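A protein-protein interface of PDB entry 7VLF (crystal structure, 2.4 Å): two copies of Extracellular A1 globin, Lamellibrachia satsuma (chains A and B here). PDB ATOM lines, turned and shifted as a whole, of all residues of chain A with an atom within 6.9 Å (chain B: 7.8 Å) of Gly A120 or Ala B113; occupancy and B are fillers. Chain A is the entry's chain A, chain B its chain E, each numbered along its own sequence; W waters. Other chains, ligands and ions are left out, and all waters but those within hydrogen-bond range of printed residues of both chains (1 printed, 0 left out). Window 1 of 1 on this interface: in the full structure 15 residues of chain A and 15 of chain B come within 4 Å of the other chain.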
ATOM      1  N   ALA A  17      23.020  13.000  14.399  1.00  0.00           N
ATOM      2  CA  ALA A  17      23.758  11.943  15.082  1.00  0.00           C
ATOM      3  C   ALA A  17      24.444  12.449  16.344  1.00  0.00           C
ATOM      4  O   ALA A  17      24.579  11.698  17.316  1.00  0.00           O
ATOM      5  CB  ALA A  17      24.786  11.326  14.135  1.00  0.00           C
ATOM      6  N   VAL A 115      29.025   7.912  13.284  1.00  0.00           N
ATOM      7  CA  VAL A 115      27.914   8.678  12.733  1.00  0.00           C
ATOM      8  C   VAL A 115      26.984   7.769  11.940  1.00  0.00           C
ATOM      9  O   VAL A 115      25.758   7.904  12.006  1.00  0.00           O
ATOM     10  CB  VAL A 115      28.434   9.845  11.873  1.00  0.00           C
ATOM     11  CG1 VAL A 115      27.273  10.657  11.329  1.00  0.00           C
ATOM     12  CG2 VAL A 115      29.358  10.731  12.683  1.00  0.00           C
ATOM     13  N   GLY A 116      27.549   6.822  11.189  1.00  0.00           N
ATOM     14  CA  GLY A 116      26.721   5.945  10.376  1.00  0.00           C
ATOM     15  C   GLY A 116      25.807   5.065  11.207  1.00  0.00           C
ATOM     16  O   GLY A 116      24.614   4.939  10.919  1.00  0.00           O
ATOM     17  N   GLY A 117      26.354   4.442  12.250  1.00  0.00           N
ATOM     18  CA  GLY A 117      25.535   3.606  13.110  1.00  0.00           C
ATOM     19  C   GLY A 117      24.542   4.396  13.933  1.00  0.00           C
ATOM     20  O   GLY A 117      23.491   3.875  14.316  1.00  0.00           O
ATOM     21  N   GLN A 118      24.847   5.660  14.214  1.00  0.00           N
ATOM     22  CA  GLN A 118      23.915   6.469  14.988  1.00  0.00           C
ATOM     23  C   GLN A 118      22.866   7.113  14.086  1.00  0.00           C
ATOM     24  O   GLN A 118      21.698   7.240  14.475  1.00  0.00           O
ATOM     25  CB  GLN A 118      24.682   7.529  15.779  1.00  0.00           C
ATOM     26  CG  GLN A 118      23.816   8.390  16.674  1.00  0.00           C
ATOM     27  CD  GLN A 118      23.089   7.590  17.732  1.00  0.00           C
ATOM     28  OE1 GLN A 118      23.659   7.234  18.763  1.00  0.00           O
ATOM     29  NE2 GLN A 118      21.814   7.311  17.489  1.00  0.00           N
ATOM     30  N   PHE A 119      23.264   7.530  12.878  1.00  0.00           N
ATOM     31  CA  PHE A 119      22.313   8.165  11.969  1.00  0.00           C
ATOM     32  C   PHE A 119      21.405   7.129  11.323  1.00  0.00           C
ATOM     33  O   PHE A 119      20.200   7.369  11.129  1.00  0.00           O
ATOM     34  CB  PHE A 119      23.059   8.961  10.904  1.00  0.00           C
ATOM     35  CG  PHE A 119      22.161   9.663   9.933  1.00  0.00           C
ATOM     36  CD1 PHE A 119      21.602  10.888  10.251  1.00  0.00           C
ATOM     37  CD2 PHE A 119      21.886   9.108   8.695  1.00  0.00           C
ATOM     38  CE1 PHE A 119      20.781  11.546   9.359  1.00  0.00           C
ATOM     39  CE2 PHE A 119      21.065   9.757   7.796  1.00  0.00           C
ATOM     40  CZ  PHE A 119      20.511  10.980   8.128  1.00  0.00           C
ATOM     41  N   GLY A 120      21.960   5.971  10.993  1.00  0.00           N
ATOM     42  CA  GLY A 120      21.196   4.898  10.410  1.00  0.00           C
ATOM     43  C   GLY A 120      21.703   4.534   9.028  1.00  0.00           C
ATOM     44  O   GLY A 120      22.840   4.807   8.644  1.00  0.00           O
ATOM     45  N   VAL A 121      20.822   3.904   8.262  1.00  0.00           N
ATOM     46  CA  VAL A 121      21.207   3.375   6.960  1.00  0.00           C
ATOM     47  C   VAL A 121      21.385   4.491   5.928  1.00  0.00           C
ATOM     48  O   VAL A 121      22.162   4.343   4.971  1.00  0.00           O
ATOM     49  CB  VAL A 121      20.160   2.336   6.520  1.00  0.00           C
ATOM     50  CG1 VAL A 121      20.555   1.700   5.209  1.00  0.00           C
ATOM     51  CG2 VAL A 121      19.994   1.276   7.594  1.00  0.00           C
ATOM     52  N   CYS A 122      20.704   5.623   6.105  1.00  0.00           N
ATOM     53  CA  CYS A 122      20.748   6.676   5.099  1.00  0.00           C
ATOM     54  C   CYS A 122      22.024   7.493   5.242  1.00  0.00           C
ATOM     55  O   CYS A 122      22.092   8.630   4.774  1.00  0.00           O
ATOM     56  CB  CYS A 122      19.523   7.598   5.207  1.00  0.00           C
ATOM     57  SG  CYS A 122      17.901   6.795   5.139  1.00  0.00           S
ATOM     58  N   PHE A 123      23.039   6.907   5.878  1.00  0.00           N
ATOM     59  CA  PHE A 123      24.316   7.579   6.051  1.00  0.00           C
ATOM     60  C   PHE A 123      25.030   7.685   4.711  1.00  0.00           C
ATOM     61  O   PHE A 123      25.233   6.681   4.021  1.00  0.00           O
ATOM     62  CB  PHE A 123      25.173   6.823   7.065  1.00  0.00           C
ATOM     63  CG  PHE A 123      26.517   7.444   7.309  1.00  0.00           C
ATOM     64  CD1 PHE A 123      26.624   8.684   7.911  1.00  0.00           C
ATOM     65  CD2 PHE A 123      27.677   6.773   6.960  1.00  0.00           C
ATOM     66  CE1 PHE A 123      27.860   9.256   8.144  1.00  0.00           C
ATOM     67  CE2 PHE A 123      28.915   7.337   7.191  1.00  0.00           C
ATOM     68  CZ  PHE A 123      29.008   8.582   7.785  1.00  0.00           C
ATOM     69  N   ASP A 124      25.390   8.909   4.331  1.00  0.00           N
ATOM     70  CA  ASP A 124      26.018   9.176   3.036  1.00  0.00           C
ATOM     71  C   ASP A 124      27.527   9.078   3.212  1.00  0.00           C
ATOM     72  O   ASP A 124      28.213  10.071   3.457  1.00  0.00           O
ATOM     73  CB  ASP A 124      25.600  10.542   2.512  1.00  0.00           C
ATOM     74  CG  ASP A 124      25.912  10.723   1.042  1.00  0.00           C
ATOM     75  OD1 ASP A 124      26.929  10.174   0.571  1.00  0.00           O
ATOM     76  OD2 ASP A 124      25.130  11.408   0.353  1.00  0.00           O
ATOM     77  N   LEU A 125      28.052   7.863   3.063  1.00  0.00           N
ATOM     78  CA  LEU A 125      29.487   7.649   3.245  1.00  0.00           C
ATOM     79  C   LEU A 125      30.346   8.399   2.232  1.00  0.00           C
ATOM     80  O   LEU A 125      31.325   9.041   2.651  1.00  0.00           O
ATOM     81  CB  LEU A 125      29.784   6.146   3.227  1.00  0.00           C
ATOM     82  CG  LEU A 125      31.261   5.756   3.297  1.00  0.00           C
ATOM     83  CD1 LEU A 125      31.873   6.203   4.616  1.00  0.00           C
ATOM     84  CD2 LEU A 125      31.436   4.258   3.099  1.00  0.00           C
ATOM     85  N   PRO A 126      30.072   8.361   0.919  1.00  0.00           N
ATOM     86  CA  PRO A 126      30.948   9.094  -0.015  1.00  0.00           C
ATOM     87  C   PRO A 126      31.012  10.585   0.255  1.00  0.00           C
ATOM     88  O   PRO A 126      32.070  11.199   0.076  1.00  0.00           O
ATOM     89  CB  PRO A 126      30.324   8.792  -1.384  1.00  0.00           C
ATOM     90  CG  PRO A 126      29.611   7.508  -1.193  1.00  0.00           C
ATOM     91  CD  PRO A 126      29.052   7.584   0.192  1.00  0.00           C
ATOM     92  N   PHE B  27      16.668  -5.002   3.617  1.00  0.00           N
ATOM     93  CA  PHE B  27      18.078  -4.632   3.677  1.00  0.00           C
ATOM     94  C   PHE B  27      18.617  -4.317   2.287  1.00  0.00           C
ATOM     95  O   PHE B  27      19.223  -3.260   2.063  1.00  0.00           O
ATOM     96  CB  PHE B  27      18.883  -5.754   4.334  1.00  0.00           C
ATOM     97  CG  PHE B  27      20.335  -5.425   4.535  1.00  0.00           C
ATOM     98  CD1 PHE B  27      21.268  -5.695   3.547  1.00  0.00           C
ATOM     99  CD2 PHE B  27      20.770  -4.857   5.720  1.00  0.00           C
ATOM    100  CE1 PHE B  27      22.605  -5.394   3.733  1.00  0.00           C
ATOM    101  CE2 PHE B  27      22.105  -4.557   5.911  1.00  0.00           C
ATOM    102  CZ  PHE B  27      23.021  -4.826   4.916  1.00  0.00           C
ATOM    103  N   SER B  30      17.350  -0.991   0.882  1.00  0.00           N
ATOM    104  CA  SER B  30      18.065   0.172   1.395  1.00  0.00           C
ATOM    105  C   SER B  30      19.427   0.314   0.730  1.00  0.00           C
ATOM    106  O   SER B  30      19.886   1.431   0.461  1.00  0.00           O
ATOM    107  CB  SER B  30      18.222   0.065   2.912  1.00  0.00           C
ATOM    108  OG  SER B  30      16.958  -0.028   3.546  1.00  0.00           O
ATOM    109  N   LEU B  31      20.088  -0.810   0.453  1.00  0.00           N
ATOM    110  CA  LEU B  31      21.396  -0.765  -0.189  1.00  0.00           C
ATOM    111  C   LEU B  31      21.281  -0.278  -1.629  1.00  0.00           C
ATOM    112  O   LEU B  31      22.015   0.624  -2.052  1.00  0.00           O
ATOM    113  CB  LEU B  31      22.046  -2.149  -0.125  1.00  0.00           C
ATOM    114  CG  LEU B  31      23.551  -2.284  -0.373  1.00  0.00           C
ATOM    115  CD1 LEU B  31      24.084  -3.510   0.349  1.00  0.00           C
ATOM    116  CD2 LEU B  31      23.863  -2.380  -1.855  1.00  0.00           C
ATOM    117  N   SER B  34      20.637   3.286  -1.904  1.00  0.00           N
ATOM    118  CA  SER B  34      21.836   4.086  -1.675  1.00  0.00           C
ATOM    119  C   SER B  34      22.744   4.086  -2.896  1.00  0.00           C
ATOM    120  O   SER B  34      23.406   5.090  -3.180  1.00  0.00           O
ATOM    121  CB  SER B  34      22.588   3.568  -0.453  1.00  0.00           C
ATOM    122  OG  SER B  34      21.771   3.636   0.701  1.00  0.00           O
ATOM    123  N   TYR B  38      23.911   7.331  -4.847  1.00  0.00           N
ATOM    124  CA  TYR B  38      25.326   7.653  -4.998  1.00  0.00           C
ATOM    125  C   TYR B  38      25.690   7.836  -6.466  1.00  0.00           C
ATOM    126  O   TYR B  38      26.353   8.812  -6.837  1.00  0.00           O
ATOM    127  CB  TYR B  38      26.188   6.557  -4.367  1.00  0.00           C
ATOM    128  CG  TYR B  38      26.087   6.454  -2.860  1.00  0.00           C
ATOM    129  CD1 TYR B  38      25.541   7.484  -2.105  1.00  0.00           C
ATOM    130  CD2 TYR B  38      26.549   5.326  -2.193  1.00  0.00           C
ATOM    131  CE1 TYR B  38      25.453   7.390  -0.727  1.00  0.00           C
ATOM    132  CE2 TYR B  38      26.467   5.224  -0.817  1.00  0.00           C
ATOM    133  CZ  TYR B  38      25.916   6.258  -0.089  1.00  0.00           C
ATOM    134  OH  TYR B  38      25.834   6.158   1.281  1.00  0.00           O
ATOM    135  N   PHE B 107      29.387   0.219  -5.018  1.00  0.00           N
ATOM    136  CA  PHE B 107      28.717  -0.890  -4.346  1.00  0.00           C
ATOM    137  C   PHE B 107      29.238  -1.066  -2.926  1.00  0.00           C
ATOM    138  O   PHE B 107      28.477  -1.409  -2.015  1.00  0.00           O
ATOM    139  CB  PHE B 107      28.903  -2.177  -5.151  1.00  0.00           C
ATOM    140  CG  PHE B 107      28.037  -3.316  -4.692  1.00  0.00           C
ATOM    141  CD1 PHE B 107      28.463  -4.170  -3.689  1.00  0.00           C
ATOM    142  CD2 PHE B 107      26.801  -3.542  -5.276  1.00  0.00           C
ATOM    143  CE1 PHE B 107      27.670  -5.219  -3.270  1.00  0.00           C
ATOM    144  CE2 PHE B 107      26.003  -4.590  -4.860  1.00  0.00           C
ATOM    145  CZ  PHE B 107      26.438  -5.430  -3.857  1.00  0.00           C
ATOM    146  N   GLY B 108      30.537  -0.836  -2.720  1.00  0.00           N
ATOM    147  CA  GLY B 108      31.100  -0.972  -1.388  1.00  0.00           C
ATOM    148  C   GLY B 108      30.642   0.121  -0.442  1.00  0.00           C
ATOM    149  O   GLY B 108      30.382  -0.136   0.736  1.00  0.00           O
ATOM    150  N   LYS B 109      30.533   1.356  -0.944  1.00  0.00           N
ATOM    151  CA  LYS B 109      30.118   2.467  -0.093  1.00  0.00           C
ATOM    152  C   LYS B 109      28.708   2.255   0.444  1.00  0.00           C
ATOM    153  O   LYS B 109      28.433   2.534   1.617  1.00  0.00           O
ATOM    154  CB  LYS B 109      30.205   3.783  -0.866  1.00  0.00           C
ATOM    155  CG  LYS B 109      31.573   4.062  -1.473  1.00  0.00           C
ATOM    156  CD  LYS B 109      32.676   3.922  -0.435  1.00  0.00           C
ATOM    157  CE  LYS B 109      34.054   4.165  -1.036  1.00  0.00           C
ATOM    158  NZ  LYS B 109      34.335   5.610  -1.264  1.00  0.00           N
ATOM    159  N   ALA B 110      27.800   1.757  -0.398  1.00  0.00           N
ATOM    160  CA  ALA B 110      26.439   1.502   0.061  1.00  0.00           C
ATOM    161  C   ALA B 110      26.391   0.313   1.010  1.00  0.00           C
ATOM    162  O   ALA B 110      25.606   0.306   1.963  1.00  0.00           O
ATOM    163  CB  ALA B 110      25.514   1.274  -1.132  1.00  0.00           C
ATOM    164  N   LEU B 111      27.223  -0.702   0.766  1.00  0.00           N
ATOM    165  CA  LEU B 111      27.251  -1.866   1.647  1.00  0.00           C
ATOM    166  C   LEU B 111      27.655  -1.475   3.062  1.00  0.00           C
ATOM    167  O   LEU B 111      27.038  -1.909   4.042  1.00  0.00           O
ATOM    168  CB  LEU B 111      28.207  -2.918   1.089  1.00  0.00           C
ATOM    169  CG  LEU B 111      28.477  -4.138   1.974  1.00  0.00           C
ATOM    170  CD1 LEU B 111      27.221  -4.977   2.150  1.00  0.00           C
ATOM    171  CD2 LEU B 111      29.613  -4.978   1.411  1.00  0.00           C
ATOM    172  N   PHE B 112      28.704  -0.661   3.188  1.00  0.00           N
ATOM    173  CA  PHE B 112      29.147  -0.224   4.507  1.00  0.00           C
ATOM    174  C   PHE B 112      28.088   0.638   5.182  1.00  0.00           C
ATOM    175  O   PHE B 112      27.851   0.514   6.390  1.00  0.00           O
ATOM    176  CB  PHE B 112      30.464   0.542   4.390  1.00  0.00           C
ATOM    177  CG  PHE B 112      31.549  -0.214   3.671  1.00  0.00           C
ATOM    178  CD1 PHE B 112      31.640  -1.594   3.766  1.00  0.00           C
ATOM    179  CD2 PHE B 112      32.480   0.463   2.897  1.00  0.00           C
ATOM    180  CE1 PHE B 112      32.639  -2.284   3.104  1.00  0.00           C
ATOM    181  CE2 PHE B 112      33.478  -0.221   2.232  1.00  0.00           C
ATOM    182  CZ  PHE B 112      33.559  -1.596   2.335  1.00  0.00           C
ATOM    183  N   ALA B 113      27.438   1.520   4.417  1.00  0.00           N
ATOM    184  CA  ALA B 113      26.433   2.403   4.998  1.00  0.00           C
ATOM    185  C   ALA B 113      25.172   1.644   5.388  1.00  0.00           C
ATOM    186  O   ALA B 113      24.439   2.082   6.282  1.00  0.00           O
ATOM    187  CB  ALA B 113      26.095   3.529   4.022  1.00  0.00           C
ATOM    188  N   THR B 114      24.906   0.512   4.740  1.00  0.00           N
ATOM    189  CA  THR B 114      23.715  -0.270   5.047  1.00  0.00           C
ATOM    190  C   THR B 114      23.951  -1.247   6.192  1.00  0.00           C
ATOM    191  O   THR B 114      23.064  -1.444   7.028  1.00  0.00           O
ATOM    192  CB  THR B 114      23.244  -1.023   3.800  1.00  0.00           C
ATOM    193  OG1 THR B 114      23.208  -0.122   2.689  1.00  0.00           O
ATOM    194  CG2 THR B 114      21.849  -1.587   4.012  1.00  0.00           C
ATOM    195  N   VAL B 115      25.131  -1.867   6.249  1.00  0.00           N
ATOM    196  CA  VAL B 115      25.447  -2.735   7.380  1.00  0.00           C
ATOM    197  C   VAL B 115      25.687  -1.902   8.632  1.00  0.00           C
ATOM    198  O   VAL B 115      25.155  -2.201   9.707  1.00  0.00           O
ATOM    199  CB  VAL B 115      26.659  -3.626   7.057  1.00  0.00           C
ATOM    200  CG1 VAL B 115      26.989  -4.515   8.243  1.00  0.00           C
ATOM    201  CG2 VAL B 115      26.389  -4.469   5.825  1.00  0.00           C
ATOM    202  N   GLY B 116      26.487  -0.842   8.511  1.00  0.00           N
ATOM    203  CA  GLY B 116      26.790  -0.018   9.670  1.00  0.00           C
ATOM    204  C   GLY B 116      25.563   0.659  10.246  1.00  0.00           C
ATOM    205  O   GLY B 116      25.360   0.677  11.464  1.00  0.00           O
ATOM    206  N   GLY B 117      24.726   1.228   9.378  1.00  0.00           N
ATOM    207  CA  GLY B 117      23.499   1.852   9.841  1.00  0.00           C
ATOM    208  C   GLY B 117      22.519   0.883  10.462  1.00  0.00           C
ATOM    209  O   GLY B 117      21.649   1.300  11.234  1.00  0.00           O
ATOM    210  N   GLN B 118      22.637  -0.403  10.141  1.00  0.00           N
ATOM    211  CA  GLN B 118      21.803  -1.438  10.737  1.00  0.00           C
ATOM    212  C   GLN B 118      22.476  -2.121  11.918  1.00  0.00           C
ATOM    213  O   GLN B 118      21.814  -2.407  12.921  1.00  0.00           O
ATOM    214  CB  GLN B 118      21.432  -2.486   9.683  1.00  0.00           C
ATOM    215  CG  GLN B 118      20.449  -3.534  10.171  1.00  0.00           C
ATOM    216  CD  GLN B 118      19.047  -2.985  10.345  1.00  0.00           C
ATOM    217  OE1 GLN B 118      18.586  -2.167   9.548  1.00  0.00           O
ATOM    218  NE2 GLN B 118      18.362  -3.431  11.391  1.00  0.00           N
ATOM    219  N   PHE B 119      23.784  -2.381  11.825  1.00  0.00           N
ATOM    220  CA  PHE B 119      24.492  -3.045  12.915  1.00  0.00           C
ATOM    221  C   PHE B 119      24.711  -2.109  14.096  1.00  0.00           C
ATOM    222  O   PHE B 119      24.763  -2.567  15.245  1.00  0.00           O
ATOM    223  CB  PHE B 119      25.832  -3.590  12.418  1.00  0.00           C
ATOM    224  CG  PHE B 119      26.612  -4.337  13.463  1.00  0.00           C
ATOM    225  CD1 PHE B 119      26.333  -5.667  13.736  1.00  0.00           C
ATOM    226  CD2 PHE B 119      27.633  -3.713  14.163  1.00  0.00           C
ATOM    227  CE1 PHE B 119      27.047  -6.356  14.690  1.00  0.00           C
ATOM    228  CE2 PHE B 119      28.352  -4.399  15.120  1.00  0.00           C
ATOM    229  CZ  PHE B 119      28.060  -5.722  15.384  1.00  0.00           C
ATOM    230  N   GLY B 120      24.845  -0.818  13.843  1.00  0.00           N
ATOM    231  CA  GLY B 120      25.014   0.161  14.892  1.00  0.00           C
ATOM    232  C   GLY B 120      26.397   0.782  14.896  1.00  0.00           C
ATOM    233  O   GLY B 120      27.128   0.772  13.901  1.00  0.00           O
ATOM    234  N   PHE B 123      30.031  -1.038  14.258  1.00  0.00           N
ATOM    235  CA  PHE B 123      30.400  -1.482  12.921  1.00  0.00           C
ATOM    236  C   PHE B 123      31.881  -1.235  12.667  1.00  0.00           C
ATOM    237  O   PHE B 123      32.380  -0.122  12.854  1.00  0.00           O
ATOM    238  CB  PHE B 123      29.548  -0.753  11.881  1.00  0.00           C
ATOM    239  CG  PHE B 123      29.911  -1.073  10.459  1.00  0.00           C
ATOM    240  CD1 PHE B 123      29.602  -2.307   9.912  1.00  0.00           C
ATOM    241  CD2 PHE B 123      30.542  -0.131   9.661  1.00  0.00           C
ATOM    242  CE1 PHE B 123      29.930  -2.600   8.600  1.00  0.00           C
ATOM    243  CE2 PHE B 123      30.871  -0.418   8.350  1.00  0.00           C
ATOM    244  CZ  PHE B 123      30.565  -1.654   7.820  1.00  0.00           C
ATOM    245  N   LEU B 125      34.339  -0.543  10.263  1.00  0.00           N
ATOM    246  CA  LEU B 125      34.533  -0.076   8.889  1.00  0.00           C
ATOM    247  C   LEU B 125      35.877  -0.509   8.308  1.00  0.00           C
ATOM    248  O   LEU B 125      35.904  -0.978   7.156  1.00  0.00           O
ATOM    249  CB  LEU B 125      34.363   1.447   8.836  1.00  0.00           C
ATOM    250  CG  LEU B 125      34.691   2.144   7.515  1.00  0.00           C
ATOM    251  CD1 LEU B 125      33.892   1.547   6.365  1.00  0.00           C
ATOM    252  CD2 LEU B 125      34.442   3.641   7.619  1.00  0.00           C
HETATM  253  O   HOH W   1      23.009   5.732   2.256  1.00  0.00           O
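O of Phe A123 is in hydrogen-bond range of OH of Tyr B38 (2.9 Å). The backbone carbonyl oxygen of Val A121 lies close to the backbone carbonyl oxygen of Ala B113, at 3.5 Å. The backbone NH (N) of Leu A125 lies within hydrogen-bond range of the side-chain hydroxyl (OH) of Tyr B38, 3.3 Å away.
The backbone carbonyl oxygen (O) of Ser B30 sits at hydrogen-bond distance from the side-chain hydroxyl (OG) of Ser B34 (2.9 Å). OG1 of Thr B114 is in hydrogen-bond range of O of Ala B110 (2.5 Å).
Gly A116 touches Gly B117. Gly A117 touches Gly B120. O of Gly A120 touches O of Ala B113, 3.9 Å away. Gly A120 touches Gly B117. Val A121 touches Ser B30. O of Phe A123 touches CB of Ala B113, 3.3 Å away. Asp A124 touches Tyr B38. Leu A125 touches Lys B109 (CD2 to CD, 3.8 Å). Phe B112 touches Leu A125 (CD2 to CD2, 3.9 Å). Tyr B38 touches Pro A126.
Gly A120 touches two residues of chain B. Of the printed residues of chain A, Ala B113 touches Gly A120 (3.9 Å), Val A121 (3.5 Å) and Phe A123 (3.3 Å). Of the printed residues of chain B, Gly A116 touches Gly B117. Of the printed residues of chain B, Phe A123 touches Tyr B38 and Ala B113. Printed residues of chain B within 4 Å of Val A121: Ser B30 (3.7 Å), Ala B113 (3.5 Å), Thr B114 (3.7 Å) and Gly B117 (3.7 Å). Phe B123 touches none of the printed residues of chain A.
Hydrophobic or aromatic side chains of chain B that line the printed part of chain A: Tyr B38, Phe B112 and Ala B113. Hydrophobic or aromatic side chains of chain A that line the printed part of chain B: Val A121, Leu A125 and Pro A126. Among the printed residues, no Asp or Glu carboxylate lies within 4 Å of a Lys or Arg side-chain nitrogen of the other chain.
Gly A116 touches Gly B117, and with the chains exchanged Gly A117 touches Gly B116. Gly A117 touches Gly B120, and with the chains exchanged Gly A120 touches Gly B117. 8 positions are printed for both chains. Of the 17 pairs that touch across the chains among the printed residues, 4 have their exchanged pair printed and touching as well.
Water W1 lies within hydrogen-bond range of OG of Ser B34 (2.9 Å), O of Phe A123 (3.0 Å), OH of Tyr B38 (3.0 Å) and O of Val A121 (3.2 Å).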
